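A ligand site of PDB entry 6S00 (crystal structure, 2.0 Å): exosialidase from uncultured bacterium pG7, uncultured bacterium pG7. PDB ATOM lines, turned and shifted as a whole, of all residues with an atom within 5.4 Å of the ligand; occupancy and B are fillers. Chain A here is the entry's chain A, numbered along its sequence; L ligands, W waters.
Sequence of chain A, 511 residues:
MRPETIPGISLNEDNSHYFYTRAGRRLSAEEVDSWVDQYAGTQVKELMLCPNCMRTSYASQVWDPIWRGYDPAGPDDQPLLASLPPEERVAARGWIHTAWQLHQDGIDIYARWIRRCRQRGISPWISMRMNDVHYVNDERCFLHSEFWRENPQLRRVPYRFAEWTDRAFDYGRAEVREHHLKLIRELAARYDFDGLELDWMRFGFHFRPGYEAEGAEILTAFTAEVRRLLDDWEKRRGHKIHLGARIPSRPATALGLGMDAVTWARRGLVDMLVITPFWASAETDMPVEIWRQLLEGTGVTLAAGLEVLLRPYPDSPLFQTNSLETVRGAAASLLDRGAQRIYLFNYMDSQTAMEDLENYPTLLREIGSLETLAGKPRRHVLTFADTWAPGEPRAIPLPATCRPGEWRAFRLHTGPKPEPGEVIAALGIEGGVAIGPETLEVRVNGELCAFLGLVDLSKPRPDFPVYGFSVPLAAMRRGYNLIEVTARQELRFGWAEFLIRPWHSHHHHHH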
ATOM      1  N   ASP A  14      16.976   9.541 -22.140  1.00  0.00           N
ATOM      2  CA  ASP A  14      17.709   9.136 -20.909  1.00  0.00           C
ATOM      3  C   ASP A  14      18.035  10.351 -20.005  1.00  0.00           C
ATOM      4  O   ASP A  14      17.878  11.489 -20.397  1.00  0.00           O
ATOM      5  CB  ASP A  14      18.937   8.297 -21.283  1.00  0.00           C
ATOM      6  CG  ASP A  14      20.201   9.063 -21.591  1.00  0.00           C
ATOM      7  OD1 ASP A  14      20.241  10.276 -21.301  1.00  0.00           O
ATOM      8  OD2 ASP A  14      21.145   8.411 -22.104  1.00  0.00           O
ATOM      9  N   ASN A  15      18.501  10.056 -18.795  1.00  0.00           N
ATOM     10  CA  ASN A  15      18.676  11.066 -17.708  1.00  0.00           C
ATOM     11  C   ASN A  15      19.867  11.995 -17.983  1.00  0.00           C
ATOM     12  O   ASN A  15      20.001  12.935 -17.192  1.00  0.00           O
ATOM     13  CB  ASN A  15      18.889  10.348 -16.358  1.00  0.00           C
ATOM     14  CG  ASN A  15      20.084   9.424 -16.407  1.00  0.00           C
ATOM     15  OD1 ASN A  15      20.079   8.452 -17.204  1.00  0.00           O
ATOM     16  ND2 ASN A  15      21.088   9.606 -15.537  1.00  0.00           N
ATOM     17  N   SER A  16      20.800  11.655 -18.879  1.00  0.00           N
ATOM     18  CA  SER A  16      22.130  12.344 -18.982  1.00  0.00           C
ATOM     19  C   SER A  16      22.432  12.992 -20.342  1.00  0.00           C
ATOM     20  O   SER A  16      23.153  14.018 -20.373  1.00  0.00           O
ATOM     21  CB  SER A  16      23.200  11.360 -18.614  1.00  0.00           C
ATOM     22  OG  SER A  16      23.290  10.293 -19.513  1.00  0.00           O
ATOM     23  N   TYR A  20      24.838  16.190 -21.414  1.00  0.00           N
ATOM     24  CA  TYR A  20      26.184  15.869 -21.967  1.00  0.00           C
ATOM     25  C   TYR A  20      26.397  16.589 -23.313  1.00  0.00           C
ATOM     26  O   TYR A  20      27.440  17.216 -23.483  1.00  0.00           O
ATOM     27  CB  TYR A  20      26.274  14.383 -22.289  1.00  0.00           C
ATOM     28  CG  TYR A  20      26.731  13.443 -21.203  1.00  0.00           C
ATOM     29  CD1 TYR A  20      27.988  13.539 -20.644  1.00  0.00           C
ATOM     30  CD2 TYR A  20      25.917  12.404 -20.789  1.00  0.00           C
ATOM     31  CE1 TYR A  20      28.417  12.645 -19.680  1.00  0.00           C
ATOM     32  CE2 TYR A  20      26.327  11.512 -19.812  1.00  0.00           C
ATOM     33  CZ  TYR A  20      27.584  11.633 -19.252  1.00  0.00           C
ATOM     34  OH  TYR A  20      27.989  10.746 -18.307  1.00  0.00           O
ATOM     35  N   CYS A  53      18.961   8.666 -12.288  1.00  0.00           N
ATOM     36  CA  CYS A  53      19.718   7.409 -12.152  1.00  0.00           C
ATOM     37  C   CYS A  53      19.761   7.242 -10.630  1.00  0.00           C
ATOM     38  O   CYS A  53      18.682   7.296 -10.030  1.00  0.00           O
ATOM     39  CB  CYS A  53      21.082   7.460 -12.831  1.00  0.00           C
ATOM     40  SG  CYS A  53      22.122   8.849 -12.335  1.00  0.00           S
ATOM     41  N   TRP A  95      27.717  17.100 -17.923  1.00  0.00           N
ATOM     42  CA  TRP A  95      26.365  16.739 -17.468  1.00  0.00           C
ATOM     43  C   TRP A  95      26.064  17.541 -16.192  1.00  0.00           C
ATOM     44  O   TRP A  95      25.050  18.275 -16.125  1.00  0.00           O
ATOM     45  CB  TRP A  95      26.252  15.191 -17.317  1.00  0.00           C
ATOM     46  CG  TRP A  95      25.070  14.647 -16.586  1.00  0.00           C
ATOM     47  CD1 TRP A  95      23.883  15.260 -16.285  1.00  0.00           C
ATOM     48  CD2 TRP A  95      24.959  13.326 -16.042  1.00  0.00           C
ATOM     49  NE1 TRP A  95      23.047  14.416 -15.592  1.00  0.00           N
ATOM     50  CE2 TRP A  95      23.664  13.184 -15.496  1.00  0.00           C
ATOM     51  CE3 TRP A  95      25.785  12.208 -16.097  1.00  0.00           C
ATOM     52  CZ2 TRP A  95      23.248  12.002 -14.892  1.00  0.00           C
ATOM     53  CZ3 TRP A  95      25.360  11.034 -15.500  1.00  0.00           C
ATOM     54  CH2 TRP A  95      24.124  10.951 -14.883  1.00  0.00           C
ATOM     55  N   ARG A 129      14.288   5.403 -13.629  1.00  0.00           N
ATOM     56  CA  ARG A 129      15.178   4.236 -13.486  1.00  0.00           C
ATOM     57  C   ARG A 129      15.049   3.741 -12.037  1.00  0.00           C
ATOM     58  O   ARG A 129      15.341   4.499 -11.092  1.00  0.00           O
ATOM     59  CB  ARG A 129      16.626   4.504 -13.888  1.00  0.00           C
ATOM     60  CG  ARG A 129      16.714   4.997 -15.316  1.00  0.00           C
ATOM     61  CD  ARG A 129      18.129   5.275 -15.734  1.00  0.00           C
ATOM     62  NE  ARG A 129      18.187   5.541 -17.157  1.00  0.00           N
ATOM     63  CZ  ARG A 129      19.201   5.257 -17.974  1.00  0.00           C
ATOM     64  NH1 ARG A 129      20.286   4.683 -17.547  1.00  0.00           N
ATOM     65  NH2 ARG A 129      19.078   5.517 -19.252  1.00  0.00           N
ATOM     66  N   ASP A 132      19.352   1.942 -11.202  1.00  0.00           N
ATOM     67  CA  ASP A 132      20.546   2.153 -12.056  1.00  0.00           C
ATOM     68  C   ASP A 132      21.817   1.861 -11.236  1.00  0.00           C
ATOM     69  O   ASP A 132      21.888   2.307 -10.090  1.00  0.00           O
ATOM     70  CB  ASP A 132      20.544   3.522 -12.718  1.00  0.00           C
ATOM     71  CG  ASP A 132      21.478   3.568 -13.909  1.00  0.00           C
ATOM     72  OD1 ASP A 132      22.701   3.611 -13.694  1.00  0.00           O
ATOM     73  OD2 ASP A 132      20.970   3.515 -15.049  1.00  0.00           O
ATOM     74  N   HIS A 134      25.133   2.087 -13.000  1.00  0.00           N
ATOM     75  CA  HIS A 134      26.340   2.514 -13.764  1.00  0.00           C
ATOM     76  C   HIS A 134      27.503   2.786 -12.811  1.00  0.00           C
ATOM     77  O   HIS A 134      27.320   3.601 -11.841  1.00  0.00           O
ATOM     78  CB  HIS A 134      26.085   3.713 -14.655  1.00  0.00           C
ATOM     79  CG  HIS A 134      25.383   3.422 -15.936  1.00  0.00           C
ATOM     80  ND1 HIS A 134      24.047   3.592 -16.083  1.00  0.00           N
ATOM     81  CD2 HIS A 134      25.834   3.004 -17.135  1.00  0.00           C
ATOM     82  CE1 HIS A 134      23.681   3.218 -17.321  1.00  0.00           C
ATOM     83  NE2 HIS A 134      24.759   2.892 -18.004  1.00  0.00           N
ATOM     84  N   TYR A 135      28.656   2.146 -13.068  1.00  0.00           N
ATOM     85  CA  TYR A 135      29.983   2.491 -12.471  1.00  0.00           C
ATOM     86  C   TYR A 135      29.998   2.200 -10.962  1.00  0.00           C
ATOM     87  O   TYR A 135      30.795   2.854 -10.231  1.00  0.00           O
ATOM     88  CB  TYR A 135      30.440   3.920 -12.795  1.00  0.00           C
ATOM     89  CG  TYR A 135      30.176   4.317 -14.227  1.00  0.00           C
ATOM     90  CD1 TYR A 135      30.611   3.565 -15.305  1.00  0.00           C
ATOM     91  CD2 TYR A 135      29.436   5.454 -14.485  1.00  0.00           C
ATOM     92  CE1 TYR A 135      30.294   3.928 -16.608  1.00  0.00           C
ATOM     93  CE2 TYR A 135      29.097   5.812 -15.779  1.00  0.00           C
ATOM     94  CZ  TYR A 135      29.523   5.059 -16.847  1.00  0.00           C
ATOM     95  OH  TYR A 135      29.152   5.503 -18.089  1.00  0.00           O
ATOM     96  N   LEU A 143      27.944   9.895  -9.792  1.00  0.00           N
ATOM     97  CA  LEU A 143      26.485   9.675 -10.031  1.00  0.00           C
ATOM     98  C   LEU A 143      25.850   8.722  -8.995  1.00  0.00           C
ATOM     99  O   LEU A 143      24.643   8.474  -9.118  1.00  0.00           O
ATOM    100  CB  LEU A 143      26.233   9.222 -11.474  1.00  0.00           C
ATOM    101  CG  LEU A 143      27.312   8.363 -12.119  1.00  0.00           C
ATOM    102  CD1 LEU A 143      27.520   7.069 -11.337  1.00  0.00           C
ATOM    103  CD2 LEU A 143      26.966   8.064 -13.566  1.00  0.00           C
ATOM    104  N   ARG A 202      16.256  -0.997 -15.736  1.00  0.00           N
ATOM    105  CA  ARG A 202      17.506  -0.309 -15.363  1.00  0.00           C
ATOM    106  C   ARG A 202      17.725  -0.628 -13.872  1.00  0.00           C
ATOM    107  O   ARG A 202      17.266   0.164 -13.039  1.00  0.00           O
ATOM    108  CB  ARG A 202      17.485   1.178 -15.739  1.00  0.00           C
ATOM    109  CG  ARG A 202      17.873   1.464 -17.181  1.00  0.00           C
ATOM    110  CD  ARG A 202      19.298   1.066 -17.518  1.00  0.00           C
ATOM    111  NE  ARG A 202      19.666   1.085 -18.930  1.00  0.00           N
ATOM    112  CZ  ARG A 202      19.120   0.315 -19.875  1.00  0.00           C
ATOM    113  NH1 ARG A 202      18.153  -0.527 -19.575  1.00  0.00           N
ATOM    114  NH2 ARG A 202      19.541   0.412 -21.120  1.00  0.00           N
ATOM    115  N   PHE A 203      18.265  -1.811 -13.542  1.00  0.00           N
ATOM    116  CA  PHE A 203      18.962  -2.754 -14.473  1.00  0.00           C
ATOM    117  C   PHE A 203      18.262  -4.118 -14.511  1.00  0.00           C
ATOM    118  O   PHE A 203      18.880  -5.074 -14.993  1.00  0.00           O
ATOM    119  CB  PHE A 203      20.422  -2.938 -14.059  1.00  0.00           C
ATOM    120  CG  PHE A 203      21.414  -1.946 -14.632  1.00  0.00           C
ATOM    121  CD1 PHE A 203      21.178  -0.587 -14.588  1.00  0.00           C
ATOM    122  CD2 PHE A 203      22.606  -2.387 -15.183  1.00  0.00           C
ATOM    123  CE1 PHE A 203      22.094   0.317 -15.100  1.00  0.00           C
ATOM    124  CE2 PHE A 203      23.518  -1.487 -15.709  1.00  0.00           C
ATOM    125  CZ  PHE A 203      23.269  -0.137 -15.658  1.00  0.00           C
ATOM    126  N   TRP A 279      20.442  -4.067 -22.693  1.00  0.00           N
ATOM    127  CA  TRP A 279      21.256  -3.011 -23.353  1.00  0.00           C
ATOM    128  C   TRP A 279      22.224  -3.621 -24.377  1.00  0.00           C
ATOM    129  O   TRP A 279      22.496  -2.953 -25.384  1.00  0.00           O
ATOM    130  CB  TRP A 279      22.099  -2.286 -22.303  1.00  0.00           C
ATOM    131  CG  TRP A 279      23.123  -1.366 -22.910  1.00  0.00           C
ATOM    132  CD1 TRP A 279      22.938  -0.062 -23.268  1.00  0.00           C
ATOM    133  CD2 TRP A 279      24.485  -1.686 -23.221  1.00  0.00           C
ATOM    134  NE1 TRP A 279      24.098   0.448 -23.771  1.00  0.00           N
ATOM    135  CE2 TRP A 279      25.062  -0.516 -23.756  1.00  0.00           C
ATOM    136  CE3 TRP A 279      25.275  -2.826 -23.086  1.00  0.00           C
ATOM    137  CZ2 TRP A 279      26.393  -0.464 -24.168  1.00  0.00           C
ATOM    138  CZ3 TRP A 279      26.593  -2.778 -23.500  1.00  0.00           C
ATOM    139  CH2 TRP A 279      27.139  -1.611 -24.025  1.00  0.00           C
ATOM    140  N   GLU A 307      16.433  -1.687 -28.364  1.00  0.00           N
ATOM    141  CA  GLU A 307      17.671  -1.037 -27.920  1.00  0.00           C
ATOM    142  C   GLU A 307      18.484  -0.635 -29.140  1.00  0.00           C
ATOM    143  O   GLU A 307      18.187  -1.125 -30.246  1.00  0.00           O
ATOM    144  CB  GLU A 307      18.486  -1.944 -27.014  1.00  0.00           C
ATOM    145  CG  GLU A 307      18.213  -1.622 -25.555  1.00  0.00           C
ATOM    146  CD  GLU A 307      18.879  -0.358 -25.055  1.00  0.00           C
ATOM    147  OE1 GLU A 307      19.590   0.281 -25.875  1.00  0.00           O
ATOM    148  OE2 GLU A 307      18.821  -0.151 -23.775  1.00  0.00           O
ATOM    149  N   PHE A 345      14.498   2.871 -26.997  1.00  0.00           N
ATOM    150  CA  PHE A 345      15.388   3.188 -25.862  1.00  0.00           C
ATOM    151  C   PHE A 345      16.775   3.378 -26.476  1.00  0.00           C
ATOM    152  O   PHE A 345      17.243   2.493 -27.298  1.00  0.00           O
ATOM    153  CB  PHE A 345      15.324   2.126 -24.757  1.00  0.00           C
ATOM    154  CG  PHE A 345      15.956   2.526 -23.434  1.00  0.00           C
ATOM    155  CD1 PHE A 345      17.325   2.542 -23.257  1.00  0.00           C
ATOM    156  CD2 PHE A 345      15.176   3.001 -22.412  1.00  0.00           C
ATOM    157  CE1 PHE A 345      17.873   2.956 -22.059  1.00  0.00           C
ATOM    158  CE2 PHE A 345      15.736   3.419 -21.212  1.00  0.00           C
ATOM    159  CZ  PHE A 345      17.078   3.359 -21.025  1.00  0.00           C
ATOM    160  N   ASN A 346      17.416   4.495 -26.100  1.00  0.00           N
ATOM    161  CA  ASN A 346      18.771   4.877 -26.579  1.00  0.00           C
ATOM    162  C   ASN A 346      18.752   5.302 -28.036  1.00  0.00           C
ATOM    163  O   ASN A 346      19.854   5.315 -28.649  1.00  0.00           O
ATOM    164  CB  ASN A 346      19.770   3.757 -26.362  1.00  0.00           C
ATOM    165  CG  ASN A 346      20.246   3.712 -24.924  1.00  0.00           C
ATOM    166  OD1 ASN A 346      20.253   4.748 -24.241  1.00  0.00           O
ATOM    167  ND2 ASN A 346      20.620   2.525 -24.493  1.00  0.00           N
ATOM    168  N   MET A 348      18.362   8.467 -29.319  1.00  0.00           N
ATOM    169  CA  MET A 348      18.280   9.914 -29.049  1.00  0.00           C
ATOM    170  C   MET A 348      18.869  10.686 -30.245  1.00  0.00           C
ATOM    171  O   MET A 348      19.214  10.014 -31.274  1.00  0.00           O
ATOM    172  CB  MET A 348      18.978  10.187 -27.699  1.00  0.00           C
ATOM    173  CG  MET A 348      18.128   9.591 -26.568  1.00  0.00           C
ATOM    174  SD  MET A 348      18.906   9.709 -24.961  1.00  0.00           S
ATOM    175  CE  MET A 348      19.816   8.156 -24.857  1.00  0.00           C
ATOM    176  N   GLN A 351      24.984  11.384 -29.882  1.00  0.00           N
ATOM    177  CA  GLN A 351      25.895  10.598 -28.998  1.00  0.00           C
ATOM    178  C   GLN A 351      25.395   9.157 -28.812  1.00  0.00           C
ATOM    179  O   GLN A 351      26.068   8.250 -29.328  1.00  0.00           O
ATOM    180  CB  GLN A 351      26.068  11.330 -27.666  1.00  0.00           C
ATOM    181  CG  GLN A 351      27.162  10.764 -26.772  1.00  0.00           C
ATOM    182  CD  GLN A 351      27.320  11.624 -25.545  1.00  0.00           C
ATOM    183  OE1 GLN A 351      28.406  12.132 -25.264  1.00  0.00           O
ATOM    184  NE2 GLN A 351      26.235  11.831 -24.829  1.00  0.00           N
ATOM    185  N   THR A 352      24.277   8.965 -28.105  1.00  0.00           N
ATOM    186  CA  THR A 352      23.608   7.648 -27.912  1.00  0.00           C
ATOM    187  C   THR A 352      22.485   7.671 -28.949  1.00  0.00           C
ATOM    188  O   THR A 352      21.418   8.226 -28.645  1.00  0.00           O
ATOM    189  CB  THR A 352      23.123   7.483 -26.478  1.00  0.00           C
ATOM    190  OG1 THR A 352      24.282   7.610 -25.648  1.00  0.00           O
ATOM    191  CG2 THR A 352      22.440   6.161 -26.232  1.00  0.00           C
HETATM  192  C1  LIG L   1      21.585   3.276 -20.750  1.00  0.00           C
HETATM  193  C2  LIG L   1      22.037   4.705 -21.096  1.00  0.00           C
HETATM  194  C3  LIG L   1      22.873   4.529 -22.356  1.00  0.00           C
HETATM  195  C4  LIG L   1      23.657   5.763 -22.799  1.00  0.00           C
HETATM  196  C5  LIG L   1      24.450   6.347 -21.626  1.00  0.00           C
HETATM  197  C6  LIG L   1      23.502   6.526 -20.440  1.00  0.00           C
HETATM  198  C7  LIG L   1      24.216   7.002 -19.184  1.00  0.00           C
HETATM  199  C8  LIG L   1      23.269   7.095 -17.994  1.00  0.00           C
HETATM  200  C9  LIG L   1      23.955   7.503 -16.691  1.00  0.00           C
HETATM  201  C10 LIG L   1      26.456   7.675 -22.173  1.00  0.00           C
HETATM  202  C11 LIG L   1      26.875   8.963 -22.805  1.00  0.00           C
HETATM  203  N1  LIG L   1      25.161   7.575 -21.928  1.00  0.00           N
HETATM  204  O1  LIG L   1      21.508   2.438 -21.560  1.00  0.00           O
HETATM  205  O2  LIG L   1      21.309   3.031 -19.644  1.00  0.00           O
HETATM  206  O3  LIG L   1      21.015   5.432 -21.607  1.00  0.00           O
HETATM  207  O4  LIG L   1      24.517   5.470 -23.882  1.00  0.00           O
HETATM  208  O5  LIG L   1      22.920   5.237 -20.137  1.00  0.00           O
HETATM  209  O6  LIG L   1      25.332   6.162 -18.915  1.00  0.00           O
HETATM  210  O7  LIG L   1      22.202   7.935 -18.286  1.00  0.00           O
HETATM  211  O8  LIG L   1      23.001   7.890 -15.717  1.00  0.00           O
HETATM  212  O9  LIG L   1      27.253   6.783 -21.934  1.00  0.00           O
HETATM  213  O   HOH W   1      23.783   6.067 -13.716  1.00  0.00           O
HETATM  214  O   HOH W   2      23.325   9.763 -22.048  1.00  0.00           O
HETATM  215  O   HOH W   3      27.200   7.815 -18.645  1.00  0.00           O
HETATM  216  O   HOH W   4      27.671   4.016 -21.051  1.00  0.00           O
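OG1 of Thr 352 is in hydrogen-bond range of O4 of the ligand, 2.8 Å away.
NE2 of His 134 sits at hydrogen-bond distance from O6 of the ligand (3.4 Å).
NE of Arg 202 is in salt-bridge range of O2 of the ligand (2.6 Å).
An oxygen (O2) of the ligand lies within salt-bridge range of the guanidinium group (NH1) of Arg 129, 2.9 Å away.
OD2 of Asp 14 is in hydrogen-bond range of O3 of the ligand (3.0 Å).
An oxygen (O7) of the ligand lies within hydrogen-bond range of the side-chain hydroxyl (OG) of Ser 16, at 2.9 Å.
The side-chain amide oxygen of Asn 15 lies within hydrogen-bond range of an oxygen (O7) of the ligand, 2.4 Å away.
The side-chain sulfur (SG) of Cys 53 sits close to an oxygen (O8) of the ligand.
The side-chain amide oxygen (OD1) of Asn 346 is in hydrogen-bond range of an oxygen (O3) of the ligand.
OD1 of Asp 132 lies within hydrogen-bond range of ND1 of His 134, at 2.7 Å.
ND2 of Asn 346 lies within hydrogen-bond range of OE1 of Glu 307 (2.8 Å).
The side-chain amide oxygen (OD1) of Asn 15 lies close to the guanidinium group (NE) of Arg 129 (3.5 Å).
N of Asp 132 is in hydrogen-bond range of O of Arg 202.
OE2 of Glu 307 lies within salt-bridge range of NH2 of Arg 202, 2.8 Å away.
NH1 of Arg 129 is in salt-bridge range of OD2 of Asp 132 (2.8 Å).
The side-chain sulfur (SG) of Cys 53 lies within hydrogen-bond range of the side-chain amide nitrogen (ND2) of Asn 15 (3.4 Å).
SD of Met 348 sits at hydrogen-bond distance from N of Asp 14.
Tyr 20 touches the ligand (CE2 to C11, 3.97 Å).
Trp 95 touches the ligand (CH2 to O8, 3.4 Å).
Tyr 135 touches the ligand.
Trp 279 touches the ligand.
Phe 345 touches the ligand (CE1 to O1, 3.7 Å).
Gln 351 touches the ligand (NE2 to C11, 3.6 Å).
Hydrophobic or aromatic side chains that line the ligand: Tyr 20, Trp 95, His 134, Trp 279 and Phe 345.
The nearest printed residue that does not touch the ligand is Glu 307 (4.3 Å).
Water W3 lies within hydrogen-bond range of an oxygen (O6) of the ligand (2.5 Å), the side-chain hydroxyl (OH) of Tyr 20 (3.1 Å) and the side-chain hydroxyl (OH) of Tyr 135 (3.1 Å).
Water W1 lies within hydrogen-bond range of OD1 of Asp 132 (2.7 Å), O8 of the ligand (2.8 Å), ND1 of His 134 (3.4 Å) and SG of Cys 53 (3.5 Å).
Water W2 lies within hydrogen-bond range of OD2 of Asp 14, OG of Ser 16 and N1 of the ligand.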
